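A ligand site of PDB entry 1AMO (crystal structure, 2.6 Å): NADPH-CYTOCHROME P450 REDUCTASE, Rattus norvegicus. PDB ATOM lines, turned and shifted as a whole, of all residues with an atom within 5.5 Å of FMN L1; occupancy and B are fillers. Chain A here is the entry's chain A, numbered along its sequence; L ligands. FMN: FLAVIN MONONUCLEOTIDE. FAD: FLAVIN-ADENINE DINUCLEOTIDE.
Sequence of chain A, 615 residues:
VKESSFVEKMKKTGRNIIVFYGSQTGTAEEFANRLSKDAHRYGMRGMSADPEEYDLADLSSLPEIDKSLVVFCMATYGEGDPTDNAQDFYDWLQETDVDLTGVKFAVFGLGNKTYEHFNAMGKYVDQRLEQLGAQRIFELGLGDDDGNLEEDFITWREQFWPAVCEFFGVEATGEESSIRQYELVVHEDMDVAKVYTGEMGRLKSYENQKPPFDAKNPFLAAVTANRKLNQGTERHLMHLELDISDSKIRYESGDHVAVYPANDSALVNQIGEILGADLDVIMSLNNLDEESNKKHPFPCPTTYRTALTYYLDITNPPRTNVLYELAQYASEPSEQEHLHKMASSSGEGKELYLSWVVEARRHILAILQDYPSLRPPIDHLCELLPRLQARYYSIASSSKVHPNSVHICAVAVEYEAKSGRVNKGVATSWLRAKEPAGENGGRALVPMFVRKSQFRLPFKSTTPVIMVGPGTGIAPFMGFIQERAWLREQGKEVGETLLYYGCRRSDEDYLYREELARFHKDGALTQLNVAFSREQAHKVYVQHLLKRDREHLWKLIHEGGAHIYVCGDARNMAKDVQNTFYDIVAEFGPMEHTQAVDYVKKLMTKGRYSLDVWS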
ATOM      1  N   GLY A  22     -35.770  -6.184 -18.532  1.00  0.00           N
ATOM      2  CA  GLY A  22     -34.365  -6.286 -18.870  1.00  0.00           C
ATOM      3  C   GLY A  22     -33.736  -6.780 -17.574  1.00  0.00           C
ATOM      4  O   GLY A  22     -33.517  -6.002 -16.646  1.00  0.00           O
ATOM      5  N   SER A  23     -33.476  -8.071 -17.492  1.00  0.00           N
ATOM      6  CA  SER A  23     -32.933  -8.652 -16.284  1.00  0.00           C
ATOM      7  C   SER A  23     -31.763  -9.589 -16.543  1.00  0.00           C
ATOM      8  O   SER A  23     -31.658 -10.193 -17.600  1.00  0.00           O
ATOM      9  CB  SER A  23     -34.061  -9.392 -15.553  1.00  0.00           C
ATOM     10  OG  SER A  23     -33.592 -10.157 -14.458  1.00  0.00           O
ATOM     11  N   GLN A  24     -30.871  -9.665 -15.562  1.00  0.00           N
ATOM     12  CA  GLN A  24     -29.699 -10.540 -15.624  1.00  0.00           C
ATOM     13  C   GLN A  24     -29.841 -11.607 -14.556  1.00  0.00           C
ATOM     14  O   GLN A  24     -29.766 -12.800 -14.840  1.00  0.00           O
ATOM     15  CB  GLN A  24     -28.411  -9.763 -15.360  1.00  0.00           C
ATOM     16  CG  GLN A  24     -27.741  -9.235 -16.589  1.00  0.00           C
ATOM     17  CD  GLN A  24     -27.142 -10.332 -17.444  1.00  0.00           C
ATOM     18  OE1 GLN A  24     -26.883 -10.114 -18.623  1.00  0.00           O
ATOM     19  NE2 GLN A  24     -26.910 -11.501 -16.860  1.00  0.00           N
ATOM     20  N   THR A  25     -30.045 -11.161 -13.317  1.00  0.00           N
ATOM     21  CA  THR A  25     -30.192 -12.061 -12.192  1.00  0.00           C
ATOM     22  C   THR A  25     -31.633 -12.134 -11.667  1.00  0.00           C
ATOM     23  O   THR A  25     -31.869 -12.310 -10.481  1.00  0.00           O
ATOM     24  CB  THR A  25     -29.165 -11.771 -11.062  1.00  0.00           C
ATOM     25  OG1 THR A  25     -29.014 -10.357 -10.890  1.00  0.00           O
ATOM     26  CG2 THR A  25     -27.803 -12.396 -11.413  1.00  0.00           C
ATOM     27  N   GLY A  26     -32.571 -11.957 -12.594  1.00  0.00           N
ATOM     28  CA  GLY A  26     -33.990 -12.055 -12.287  1.00  0.00           C
ATOM     29  C   GLY A  26     -34.726 -11.091 -11.377  1.00  0.00           C
ATOM     30  O   GLY A  26     -35.812 -11.435 -10.921  1.00  0.00           O
ATOM     31  N   THR A  27     -34.211  -9.893 -11.138  1.00  0.00           N
ATOM     32  CA  THR A  27     -34.935  -8.977 -10.263  1.00  0.00           C
ATOM     33  C   THR A  27     -35.977  -8.181 -11.046  1.00  0.00           C
ATOM     34  O   THR A  27     -37.112  -8.019 -10.590  1.00  0.00           O
ATOM     35  CB  THR A  27     -33.998  -8.027  -9.484  1.00  0.00           C
ATOM     36  OG1 THR A  27     -33.012  -8.801  -8.778  1.00  0.00           O
ATOM     37  CG2 THR A  27     -34.780  -7.223  -8.469  1.00  0.00           C
ATOM     38  N   ALA A  28     -35.598  -7.695 -12.217  1.00  0.00           N
ATOM     39  CA  ALA A  28     -36.506  -6.930 -13.064  1.00  0.00           C
ATOM     40  C   ALA A  28     -37.670  -7.822 -13.484  1.00  0.00           C
ATOM     41  O   ALA A  28     -38.790  -7.350 -13.662  1.00  0.00           O
ATOM     42  CB  ALA A  28     -35.750  -6.403 -14.291  1.00  0.00           C
ATOM     43  N   GLU A  29     -37.404  -9.117 -13.639  1.00  0.00           N
ATOM     44  CA  GLU A  29     -38.454 -10.058 -14.013  1.00  0.00           C
ATOM     45  C   GLU A  29     -39.450 -10.175 -12.868  1.00  0.00           C
ATOM     46  O   GLU A  29     -40.644 -10.043 -13.083  1.00  0.00           O
ATOM     47  CB  GLU A  29     -37.897 -11.450 -14.316  1.00  0.00           C
ATOM     48  CG  GLU A  29     -38.971 -12.370 -14.888  1.00  0.00           C
ATOM     49  CD  GLU A  29     -38.535 -13.820 -14.990  1.00  0.00           C
ATOM     50  OE1 GLU A  29     -37.401 -14.081 -15.444  1.00  0.00           O
ATOM     51  OE2 GLU A  29     -39.349 -14.696 -14.631  1.00  0.00           O
ATOM     52  N   ALA A  75     -32.869  -3.159 -16.045  1.00  0.00           N
ATOM     53  CA  ALA A  75     -31.696  -3.162 -15.185  1.00  0.00           C
ATOM     54  C   ALA A  75     -30.495  -2.709 -16.016  1.00  0.00           C
ATOM     55  O   ALA A  75     -30.433  -2.977 -17.225  1.00  0.00           O
ATOM     56  CB  ALA A  75     -31.444  -4.566 -14.618  1.00  0.00           C
ATOM     57  N   THR A  76     -29.570  -2.005 -15.390  1.00  0.00           N
ATOM     58  CA  THR A  76     -28.367  -1.535 -16.066  1.00  0.00           C
ATOM     59  C   THR A  76     -27.168  -2.290 -15.516  1.00  0.00           C
ATOM     60  O   THR A  76     -27.017  -2.453 -14.308  1.00  0.00           O
ATOM     61  CB  THR A  76     -28.191  -0.007 -15.898  1.00  0.00           C
ATOM     62  OG1 THR A  76     -26.838   0.359 -16.173  1.00  0.00           O
ATOM     63  CG2 THR A  76     -28.549   0.411 -14.500  1.00  0.00           C
ATOM     64  N   TYR A  77     -26.279  -2.721 -16.441  1.00  0.00           N
ATOM     65  CA  TYR A  77     -25.125  -3.542 -16.017  1.00  0.00           C
ATOM     66  C   TYR A  77     -23.824  -3.061 -16.664  1.00  0.00           C
ATOM     67  O   TYR A  77     -23.827  -2.507 -17.770  1.00  0.00           O
ATOM     68  CB  TYR A  77     -25.345  -5.002 -16.449  1.00  0.00           C
ATOM     69  CG  TYR A  77     -25.964  -5.852 -15.350  1.00  0.00           C
ATOM     70  CD1 TYR A  77     -27.337  -5.788 -15.135  1.00  0.00           C
ATOM     71  CD2 TYR A  77     -25.153  -6.686 -14.581  1.00  0.00           C
ATOM     72  CE1 TYR A  77     -27.907  -6.556 -14.113  1.00  0.00           C
ATOM     73  CE2 TYR A  77     -25.723  -7.454 -13.559  1.00  0.00           C
ATOM     74  CZ  TYR A  77     -27.103  -7.391 -13.322  1.00  0.00           C
ATOM     75  OH  TYR A  77     -27.660  -8.116 -12.315  1.00  0.00           O
ATOM     76  N   GLY A  78     -22.737  -3.270 -15.937  1.00  0.00           N
ATOM     77  CA  GLY A  78     -21.356  -2.936 -16.414  1.00  0.00           C
ATOM     78  C   GLY A  78     -21.023  -1.437 -16.330  1.00  0.00           C
ATOM     79  O   GLY A  78     -20.857  -0.887 -15.236  1.00  0.00           O
ATOM     80  N   GLU A  79     -20.931  -0.845 -17.519  1.00  0.00           N
ATOM     81  CA  GLU A  79     -20.615   0.592 -17.698  1.00  0.00           C
ATOM     82  C   GLU A  79     -21.860   1.332 -18.225  1.00  0.00           C
ATOM     83  O   GLU A  79     -21.761   2.195 -19.108  1.00  0.00           O
ATOM     84  CB  GLU A  79     -19.460   0.758 -18.711  1.00  0.00           C
ATOM     85  CG  GLU A  79     -18.107   0.308 -18.152  1.00  0.00           C
ATOM     86  CD  GLU A  79     -16.952   0.478 -19.137  1.00  0.00           C
ATOM     87  OE1 GLU A  79     -16.837   1.561 -19.820  1.00  0.00           O
ATOM     88  OE2 GLU A  79     -16.091  -0.467 -19.287  1.00  0.00           O
ATOM     89  N   GLY A  80     -22.996   0.978 -17.639  1.00  0.00           N
ATOM     90  CA  GLY A  80     -24.265   1.583 -18.008  1.00  0.00           C
ATOM     91  C   GLY A  80     -24.814   0.957 -19.277  1.00  0.00           C
ATOM     92  O   GLY A  80     -25.459   1.615 -20.085  1.00  0.00           O
ATOM     93  N   ASP A  81     -24.518  -0.322 -19.455  1.00  0.00           N
ATOM     94  CA  ASP A  81     -24.973  -1.061 -20.624  1.00  0.00           C
ATOM     95  C   ASP A  81     -26.230  -1.852 -20.282  1.00  0.00           C
ATOM     96  O   ASP A  81     -26.546  -2.037 -19.110  1.00  0.00           O
ATOM     97  CB  ASP A  81     -23.872  -2.003 -21.113  1.00  0.00           C
ATOM     98  CG  ASP A  81     -22.701  -1.263 -21.743  1.00  0.00           C
ATOM     99  OD1 ASP A  81     -22.746  -1.032 -22.974  1.00  0.00           O
ATOM    100  OD2 ASP A  81     -21.749  -0.928 -21.018  1.00  0.00           O
ATOM    101  N   THR A  83     -28.874  -5.213 -20.167  1.00  0.00           N
ATOM    102  CA  THR A  83     -28.674  -6.593 -19.807  1.00  0.00           C
ATOM    103  C   THR A  83     -28.683  -7.416 -21.102  1.00  0.00           C
ATOM    104  O   THR A  83     -29.233  -6.976 -22.115  1.00  0.00           O
ATOM    105  CB  THR A  83     -29.796  -7.077 -18.911  1.00  0.00           C
ATOM    106  OG1 THR A  83     -31.047  -6.705 -19.483  1.00  0.00           O
ATOM    107  CG2 THR A  83     -29.678  -6.457 -17.535  1.00  0.00           C
ATOM    108  N   LEU A 110     -33.703  -0.308 -12.415  1.00  0.00           N
ATOM    109  CA  LEU A 110     -33.114  -1.061 -11.313  1.00  0.00           C
ATOM    110  C   LEU A 110     -31.622  -0.777 -11.413  1.00  0.00           C
ATOM    111  O   LEU A 110     -31.010  -1.014 -12.449  1.00  0.00           O
ATOM    112  CB  LEU A 110     -33.359  -2.573 -11.464  1.00  0.00           C
ATOM    113  CG  LEU A 110     -34.707  -3.173 -11.084  1.00  0.00           C
ATOM    114  CD1 LEU A 110     -35.784  -2.758 -12.062  1.00  0.00           C
ATOM    115  CD2 LEU A 110     -34.576  -4.684 -11.040  1.00  0.00           C
ATOM    116  N   GLY A 111     -31.046  -0.219 -10.346  1.00  0.00           N
ATOM    117  CA  GLY A 111     -29.637   0.097 -10.368  1.00  0.00           C
ATOM    118  C   GLY A 111     -28.974   0.019  -9.012  1.00  0.00           C
ATOM    119  O   GLY A 111     -29.492  -0.598  -8.094  1.00  0.00           O
ATOM    120  N   ASN A 112     -27.817   0.654  -8.892  1.00  0.00           N
ATOM    121  CA  ASN A 112     -27.064   0.667  -7.643  1.00  0.00           C
ATOM    122  C   ASN A 112     -26.148   1.879  -7.692  1.00  0.00           C
ATOM    123  O   ASN A 112     -25.292   1.963  -8.562  1.00  0.00           O
ATOM    124  CB  ASN A 112     -26.232  -0.618  -7.528  1.00  0.00           C
ATOM    125  CG  ASN A 112     -25.658  -0.826  -6.145  1.00  0.00           C
ATOM    126  OD1 ASN A 112     -25.595   0.102  -5.354  1.00  0.00           O
ATOM    127  ND2 ASN A 112     -25.275  -2.055  -5.849  1.00  0.00           N
ATOM    128  N   LYS A 113     -26.337   2.797  -6.747  1.00  0.00           N
ATOM    129  CA  LYS A 113     -25.545   4.029  -6.687  1.00  0.00           C
ATOM    130  C   LYS A 113     -24.037   3.822  -6.581  1.00  0.00           C
ATOM    131  O   LYS A 113     -23.273   4.653  -7.063  1.00  0.00           O
ATOM    132  CB  LYS A 113     -26.027   4.949  -5.563  1.00  0.00           C
ATOM    133  CG  LYS A 113     -27.361   5.597  -5.861  1.00  0.00           C
ATOM    134  CD  LYS A 113     -27.772   6.549  -4.762  1.00  0.00           C
ATOM    135  CE  LYS A 113     -29.185   7.083  -4.978  1.00  0.00           C
ATOM    136  NZ  LYS A 113     -29.308   7.939  -6.202  1.00  0.00           N
ATOM    137  N   TYR A 115     -22.274   2.237  -8.295  1.00  0.00           N
ATOM    138  CA  TYR A 115     -21.732   2.188  -9.651  1.00  0.00           C
ATOM    139  C   TYR A 115     -21.903   3.596 -10.231  1.00  0.00           C
ATOM    140  O   TYR A 115     -22.751   4.363  -9.764  1.00  0.00           O
ATOM    141  CB  TYR A 115     -22.460   1.137 -10.487  1.00  0.00           C
ATOM    142  CG  TYR A 115     -22.301  -0.271  -9.929  1.00  0.00           C
ATOM    143  CD1 TYR A 115     -23.148  -0.743  -8.928  1.00  0.00           C
ATOM    144  CD2 TYR A 115     -21.274  -1.094 -10.368  1.00  0.00           C
ATOM    145  CE1 TYR A 115     -22.969  -2.015  -8.371  1.00  0.00           C
ATOM    146  CE2 TYR A 115     -21.083  -2.372  -9.817  1.00  0.00           C
ATOM    147  CZ  TYR A 115     -21.930  -2.820  -8.821  1.00  0.00           C
ATOM    148  OH  TYR A 115     -21.733  -4.052  -8.248  1.00  0.00           O
ATOM    149  N   GLU A 116     -21.103   3.949 -11.234  1.00  0.00           N
ATOM    150  CA  GLU A 116     -21.153   5.292 -11.822  1.00  0.00           C
ATOM    151  C   GLU A 116     -22.374   5.660 -12.651  1.00  0.00           C
ATOM    152  O   GLU A 116     -22.939   6.753 -12.477  1.00  0.00           O
ATOM    153  CB  GLU A 116     -19.886   5.556 -12.655  1.00  0.00           C
ATOM    154  CG  GLU A 116     -18.638   5.833 -11.820  1.00  0.00           C
ATOM    155  CD  GLU A 116     -17.411   6.091 -12.675  1.00  0.00           C
ATOM    156  OE1 GLU A 116     -17.002   5.165 -13.420  1.00  0.00           O
ATOM    157  OE2 GLU A 116     -16.857   7.209 -12.608  1.00  0.00           O
ATOM    158  N   HIS A 117     -22.758   4.775 -13.550  1.00  0.00           N
ATOM    159  CA  HIS A 117     -23.893   4.996 -14.432  1.00  0.00           C
ATOM    160  C   HIS A 117     -25.193   4.484 -13.822  1.00  0.00           C
ATOM    161  O   HIS A 117     -25.841   3.572 -14.342  1.00  0.00           O
ATOM    162  CB  HIS A 117     -23.602   4.343 -15.785  1.00  0.00           C
ATOM    163  CG  HIS A 117     -22.227   4.655 -16.301  1.00  0.00           C
ATOM    164  ND1 HIS A 117     -22.001   5.509 -17.366  1.00  0.00           N
ATOM    165  CD2 HIS A 117     -21.008   4.260 -15.869  1.00  0.00           C
ATOM    166  CE1 HIS A 117     -20.701   5.633 -17.558  1.00  0.00           C
ATOM    167  NE2 HIS A 117     -20.071   4.881 -16.663  1.00  0.00           N
ATOM    168  N   PHE A 118     -25.581   5.111 -12.704  1.00  0.00           N
ATOM    169  CA  PHE A 118     -26.773   4.762 -11.947  1.00  0.00           C
ATOM    170  C   PHE A 118     -28.033   4.782 -12.790  1.00  0.00           C
ATOM    171  O   PHE A 118     -28.479   5.857 -13.219  1.00  0.00           O
ATOM    172  CB  PHE A 118     -26.927   5.722 -10.772  1.00  0.00           C
ATOM    173  CG  PHE A 118     -28.131   5.454  -9.929  1.00  0.00           C
ATOM    174  CD1 PHE A 118     -28.271   4.256  -9.241  1.00  0.00           C
ATOM    175  CD2 PHE A 118     -29.107   6.417  -9.785  1.00  0.00           C
ATOM    176  CE1 PHE A 118     -29.382   4.025  -8.417  1.00  0.00           C
ATOM    177  CE2 PHE A 118     -30.223   6.205  -8.971  1.00  0.00           C
ATOM    178  CZ  PHE A 118     -30.358   4.999  -8.282  1.00  0.00           C
ATOM    179  N   ASN A 119     -28.630   3.611 -12.978  1.00  0.00           N
ATOM    180  CA  ASN A 119     -29.860   3.465 -13.764  1.00  0.00           C
ATOM    181  C   ASN A 119     -29.700   4.082 -15.142  1.00  0.00           C
ATOM    182  O   ASN A 119     -30.641   4.675 -15.666  1.00  0.00           O
ATOM    183  CB  ASN A 119     -31.047   4.084 -13.035  1.00  0.00           C
ATOM    184  CG  ASN A 119     -31.683   3.128 -12.055  1.00  0.00           C
ATOM    185  OD1 ASN A 119     -31.639   1.916 -12.265  1.00  0.00           O
ATOM    186  ND2 ASN A 119     -32.262   3.651 -10.995  1.00  0.00           N
ATOM    187  N   ALA A 120     -28.509   3.962 -15.711  1.00  0.00           N
ATOM    188  CA  ALA A 120     -28.252   4.522 -17.019  1.00  0.00           C
ATOM    189  C   ALA A 120     -29.177   3.899 -18.069  1.00  0.00           C
ATOM    190  O   ALA A 120     -29.692   4.587 -18.936  1.00  0.00           O
ATOM    191  CB  ALA A 120     -26.802   4.310 -17.388  1.00  0.00           C
ATOM    192  N   ASP A 145     -30.392  -0.414  -5.549  1.00  0.00           N
ATOM    193  CA  ASP A 145     -30.001  -1.641  -4.873  1.00  0.00           C
ATOM    194  C   ASP A 145     -29.045  -1.393  -3.709  1.00  0.00           C
ATOM    195  O   ASP A 145     -28.850  -2.282  -2.865  1.00  0.00           O
ATOM    196  CB  ASP A 145     -29.391  -2.634  -5.867  1.00  0.00           C
ATOM    197  CG  ASP A 145     -29.489  -4.065  -5.404  1.00  0.00           C
ATOM    198  OD1 ASP A 145     -30.314  -4.356  -4.506  1.00  0.00           O
ATOM    199  OD2 ASP A 145     -28.755  -4.914  -5.953  1.00  0.00           O
ATOM    200  N   LEU A 149     -33.954  -1.774  -3.090  1.00  0.00           N
ATOM    201  CA  LEU A 149     -34.685  -1.823  -4.347  1.00  0.00           C
ATOM    202  C   LEU A 149     -36.140  -2.209  -4.136  1.00  0.00           C
ATOM    203  O   LEU A 149     -37.028  -1.720  -4.827  1.00  0.00           O
ATOM    204  CB  LEU A 149     -34.012  -2.801  -5.299  1.00  0.00           C
ATOM    205  CG  LEU A 149     -34.443  -2.852  -6.757  1.00  0.00           C
ATOM    206  CD1 LEU A 149     -34.353  -1.468  -7.377  1.00  0.00           C
ATOM    207  CD2 LEU A 149     -33.544  -3.822  -7.511  1.00  0.00           C
ATOM    208  N   VAL A 613     -15.560  -4.676 -10.368  1.00  0.00           N
ATOM    209  CA  VAL A 613     -15.982  -4.586  -8.980  1.00  0.00           C
ATOM    210  C   VAL A 613     -17.350  -5.194  -8.700  1.00  0.00           C
ATOM    211  O   VAL A 613     -18.144  -5.407  -9.615  1.00  0.00           O
ATOM    212  CB  VAL A 613     -15.970  -3.120  -8.540  1.00  0.00           C
ATOM    213  CG1 VAL A 613     -14.580  -2.537  -8.772  1.00  0.00           C
ATOM    214  CG2 VAL A 613     -17.017  -2.327  -9.315  1.00  0.00           C
HETATM  215  N1  FMN L   1     -26.381  -0.564 -11.587  1.00  0.00           N
HETATM  216  C2  FMN L   1     -26.325   0.650 -12.136  1.00  0.00           C
HETATM  217  O2  FMN L   1     -27.139   1.522 -11.829  1.00  0.00           O
HETATM  218  N3  FMN L   1     -25.323   0.829 -13.040  1.00  0.00           N
HETATM  219  C4  FMN L   1     -24.374  -0.101 -13.434  1.00  0.00           C
HETATM  220  O4  FMN L   1     -23.579   0.184 -14.318  1.00  0.00           O
HETATM  221  C4A FMN L   1     -24.480  -1.371 -12.798  1.00  0.00           C
HETATM  222  N5  FMN L   1     -23.526  -2.263 -13.134  1.00  0.00           N
HETATM  223  C5A FMN L   1     -23.661  -3.418 -12.439  1.00  0.00           C
HETATM  224  C6  FMN L   1     -22.659  -4.380 -12.669  1.00  0.00           C
HETATM  225  C7  FMN L   1     -22.643  -5.560 -12.009  1.00  0.00           C
HETATM  226  C7M FMN L   1     -21.537  -6.553 -12.260  1.00  0.00           C
HETATM  227  C8  FMN L   1     -23.641  -5.831 -11.082  1.00  0.00           C
HETATM  228  C8M FMN L   1     -23.630  -7.124 -10.282  1.00  0.00           C
HETATM  229  C9  FMN L   1     -24.609  -4.944 -10.853  1.00  0.00           C
HETATM  230  C9A FMN L   1     -24.649  -3.739 -11.496  1.00  0.00           C
HETATM  231  N10 FMN L   1     -25.628  -2.781 -11.236  1.00  0.00           N
HETATM  232  C10 FMN L   1     -25.522  -1.528 -11.892  1.00  0.00           C
HETATM  233  C1' FMN L   1     -26.770  -3.128 -10.386  1.00  0.00           C
HETATM  234  C2' FMN L   1     -27.957  -3.909 -10.984  1.00  0.00           C
HETATM  235  O2' FMN L   1     -28.565  -3.242 -12.080  1.00  0.00           O
HETATM  236  C3' FMN L   1     -29.023  -4.171  -9.895  1.00  0.00           C
HETATM  237  O3' FMN L   1     -28.583  -5.159  -8.971  1.00  0.00           O
HETATM  238  C4' FMN L   1     -30.376  -4.704 -10.388  1.00  0.00           C
HETATM  239  O4' FMN L   1     -31.223  -4.944  -9.262  1.00  0.00           O
HETATM  240  C5' FMN L   1     -30.209  -6.010 -11.160  1.00  0.00           C
HETATM  241  O5' FMN L   1     -31.448  -6.573 -11.652  1.00  0.00           O
HETATM  242  P   FMN L   1     -31.518  -8.029 -12.282  1.00  0.00           P
HETATM  243  O1P FMN L   1     -32.774  -7.979 -13.044  1.00  0.00           O
HETATM  244  O2P FMN L   1     -31.533  -8.902 -11.108  1.00  0.00           O
HETATM  245  O3P FMN L   1     -30.325  -8.089 -13.134  1.00  0.00           O
HETATM  246  PA  FAD L   2     -25.136 -15.769  -1.023  1.00  0.00           P
HETATM  247  O1A FAD L   2     -25.936 -16.853  -0.449  1.00  0.00           O
HETATM  248  O2A FAD L   2     -25.509 -15.091  -2.273  1.00  0.00           O
HETATM  249  O5B FAD L   2     -25.072 -14.656   0.103  1.00  0.00           O
HETATM  250  C5B FAD L   2     -24.473 -13.431  -0.221  1.00  0.00           C
HETATM  251  C4B FAD L   2     -25.183 -12.270   0.463  1.00  0.00           C
HETATM  252  O4B FAD L   2     -25.140 -12.356   1.892  1.00  0.00           O
HETATM  253  C3B FAD L   2     -24.450 -10.970   0.180  1.00  0.00           C
HETATM  254  O3B FAD L   2     -24.680 -10.598  -1.201  1.00  0.00           O
HETATM  255  C2B FAD L   2     -25.265 -10.132   1.167  1.00  0.00           C
HETATM  256  O2B FAD L   2     -26.602 -10.089   0.605  1.00  0.00           O
HETATM  257  C1B FAD L   2     -25.213 -11.033   2.412  1.00  0.00           C
HETATM  258  N9A FAD L   2     -24.076 -10.896   3.426  1.00  0.00           N
HETATM  259  C8A FAD L   2     -22.779 -11.416   3.422  1.00  0.00           C
HETATM  260  N7A FAD L   2     -22.113 -11.299   4.558  1.00  0.00           N
HETATM  261  C5A FAD L   2     -23.007 -10.631   5.393  1.00  0.00           C
HETATM  262  C6A FAD L   2     -22.919 -10.199   6.728  1.00  0.00           C
HETATM  263  N6A FAD L   2     -21.880 -10.418   7.520  1.00  0.00           N
HETATM  264  N1A FAD L   2     -23.985  -9.574   7.236  1.00  0.00           N
HETATM  265  C2A FAD L   2     -25.066  -9.378   6.482  1.00  0.00           C
HETATM  266  N3A FAD L   2     -25.277  -9.742   5.233  1.00  0.00           N
HETATM  267  C4A FAD L   2     -24.199 -10.373   4.719  1.00  0.00           C
HETATM  268  N1  FAD L   2     -16.635 -13.518  -5.234  1.00  0.00           N
HETATM  269  C2  FAD L   2     -15.462 -14.070  -4.884  1.00  0.00           C
HETATM  270  O2  FAD L   2     -15.326 -14.634  -3.795  1.00  0.00           O
HETATM  271  N3  FAD L   2     -14.507 -14.033  -5.851  1.00  0.00           N
HETATM  272  C4  FAD L   2     -14.633 -13.487  -7.138  1.00  0.00           C
HETATM  273  O4  FAD L   2     -13.684 -13.529  -7.912  1.00  0.00           O
HETATM  274  C4X FAD L   2     -15.892 -12.917  -7.471  1.00  0.00           C
HETATM  275  N5  FAD L   2     -16.013 -12.387  -8.733  1.00  0.00           N
HETATM  276  C5X FAD L   2     -17.252 -11.871  -8.964  1.00  0.00           C
HETATM  277  C6  FAD L   2     -17.419 -11.258 -10.205  1.00  0.00           C
HETATM  278  C7  FAD L   2     -18.560 -10.628 -10.582  1.00  0.00           C
HETATM  279  C7M FAD L   2     -18.636  -9.918 -11.903  1.00  0.00           C
HETATM  280  C8  FAD L   2     -19.662 -10.587  -9.718  1.00  0.00           C
HETATM  281  C8M FAD L   2     -20.897  -9.842 -10.181  1.00  0.00           C
HETATM  282  C9  FAD L   2     -19.559 -11.184  -8.481  1.00  0.00           C
HETATM  283  C9A FAD L   2     -18.343 -11.832  -8.077  1.00  0.00           C
HETATM  284  N10 FAD L   2     -18.125 -12.401  -6.792  1.00  0.00           N
HETATM  285  C10 FAD L   2     -16.843 -12.968  -6.466  1.00  0.00           C
HETATM  286  C1' FAD L   2     -19.157 -12.470  -5.778  1.00  0.00           C
HETATM  287  C2' FAD L   2     -19.821 -13.835  -5.971  1.00  0.00           C
HETATM  288  O2' FAD L   2     -20.511 -13.871  -7.243  1.00  0.00           O
HETATM  289  C3' FAD L   2     -20.796 -14.110  -4.827  1.00  0.00           C
HETATM  290  O3' FAD L   2     -21.535 -12.989  -4.382  1.00  0.00           O
HETATM  291  C4' FAD L   2     -20.108 -14.649  -3.594  1.00  0.00           C
HETATM  292  O4' FAD L   2     -19.324 -15.753  -3.984  1.00  0.00           O
HETATM  293  C5' FAD L   2     -21.153 -15.063  -2.543  1.00  0.00           C
HETATM  294  O5' FAD L   2     -22.222 -15.904  -3.042  1.00  0.00           O
HETATM  295  P   FAD L   2     -22.926 -17.010  -2.146  1.00  0.00           P
HETATM  296  O1P FAD L   2     -23.900 -17.777  -2.928  1.00  0.00           O
HETATM  297  O2P FAD L   2     -21.870 -17.737  -1.446  1.00  0.00           O
HETATM  298  O3P FAD L   2     -23.687 -16.242  -1.074  1.00  0.00           O
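OG of Ser 23 sits at hydrogen-bond distance from O1P of FMN L1, 2.7 Å away.
An oxygen (O2P) of FMN L1 lies within hydrogen-bond range of the backbone NH of Thr 27 (2.9 Å).
OG1 of Thr 27 is in hydrogen-bond range of O2P of FMN L1 (2.8 Å).
OH of Tyr 77 lies within hydrogen-bond range of O3P of FMN L1 (2.8 Å).
An oxygen (O2) of FMN L1 lies within hydrogen-bond range of the backbone NH (N) of Asn 119 (2.8 Å).
O of Thr 76 is in hydrogen-bond range of O2' of FMN L1, 2.8 Å away.
O3P of FMN L1 sits at hydrogen-bond distance from N of Thr 25 (3.1 Å).
An oxygen (O2P) of FMN L1 lies within hydrogen-bond range of the side-chain hydroxyl (OG1) of Thr 25, 2.9 Å away.
N of Gln 24 lies within hydrogen-bond range of O3P of FMN L1, 2.9 Å away.
The backbone NH of Ala 28 lies within hydrogen-bond range of an oxygen (O1P) of FMN L1 (3.0 Å).
The side-chain carboxylate of Asp 145 lies within hydrogen-bond range of an oxygen (O3') of FMN L1 (3.0 Å).
The backbone NH of Gly 78 sits at hydrogen-bond distance from a nitrogen (N5) of FMN L1, at 3.1 Å.
O of His 117 sits at hydrogen-bond distance from N3 of FMN L1 (3.1 Å).
The backbone NH (N) of Asn 112 lies within hydrogen-bond range of an oxygen (O2) of FMN L1 (3.1 Å).
O2' of FMN L1 sits at hydrogen-bond distance from O of Leu 110 (3.3 Å).
An oxygen (O4) of FMN L1 is in hydrogen-bond range of the backbone NH (N) of Gly 80, at 3.5 Å.
OG of Ser 23 sits at hydrogen-bond distance from N of Thr 27, at 3.4 Å.
The side-chain hydroxyl of Ser 23 sits at hydrogen-bond distance from the backbone NH of Gly 26 (2.8 Å).
The side-chain hydroxyl (OG1) of Thr 83 lies within hydrogen-bond range of the backbone NH (N) of Ser 23, 3.4 Å away.
The side-chain hydroxyl (OG1) of Thr 25 sits at hydrogen-bond distance from the side-chain hydroxyl (OH) of Tyr 77 (3.0 Å).
The side-chain amide oxygen of Asn 119 lies within hydrogen-bond range of the backbone NH of Gly 111 (2.9 Å).
The backbone carbonyl oxygen (O) of Leu 110 is in hydrogen-bond range of the backbone NH (N) of Thr 76, 3.4 Å away.
The backbone carbonyl oxygen (O) of Gly 111 lies within hydrogen-bond range of the backbone NH (N) of Asp 145, 2.7 Å away.
The backbone NH (N) of Ala 75 is in hydrogen-bond range of the backbone carbonyl oxygen (O) of Gly 22 (3.0 Å).
Residues that only touch FMN L1: Gly 26 (3.6 Å), Ala 75 (3.6 Å), Gly 111 (3.2 Å), Tyr 115 (3.7 Å), Phe 118 (3.3 Å) and Leu 149 (3.1 Å).
Hydrophobic or aromatic side chains that line FMN L1: Ala 28, Ala 75, Tyr 77, Leu 110, Tyr 115, Phe 118 and Leu 149.
Within 4 Å of FMN L1: Ser 23, Gln 24, Thr 25, Gly 26, Thr 27, Ala 28, Ala 75, Thr 76, Tyr 77, Gly 78, Gly 80, Leu 110, Gly 111, Asn 112, Tyr 115, His 117, Phe 118, Asn 119, Asp 145 and Leu 149.
The nearest printed residue that does not touch FMN L1 is Gly 22 (4.2 Å).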
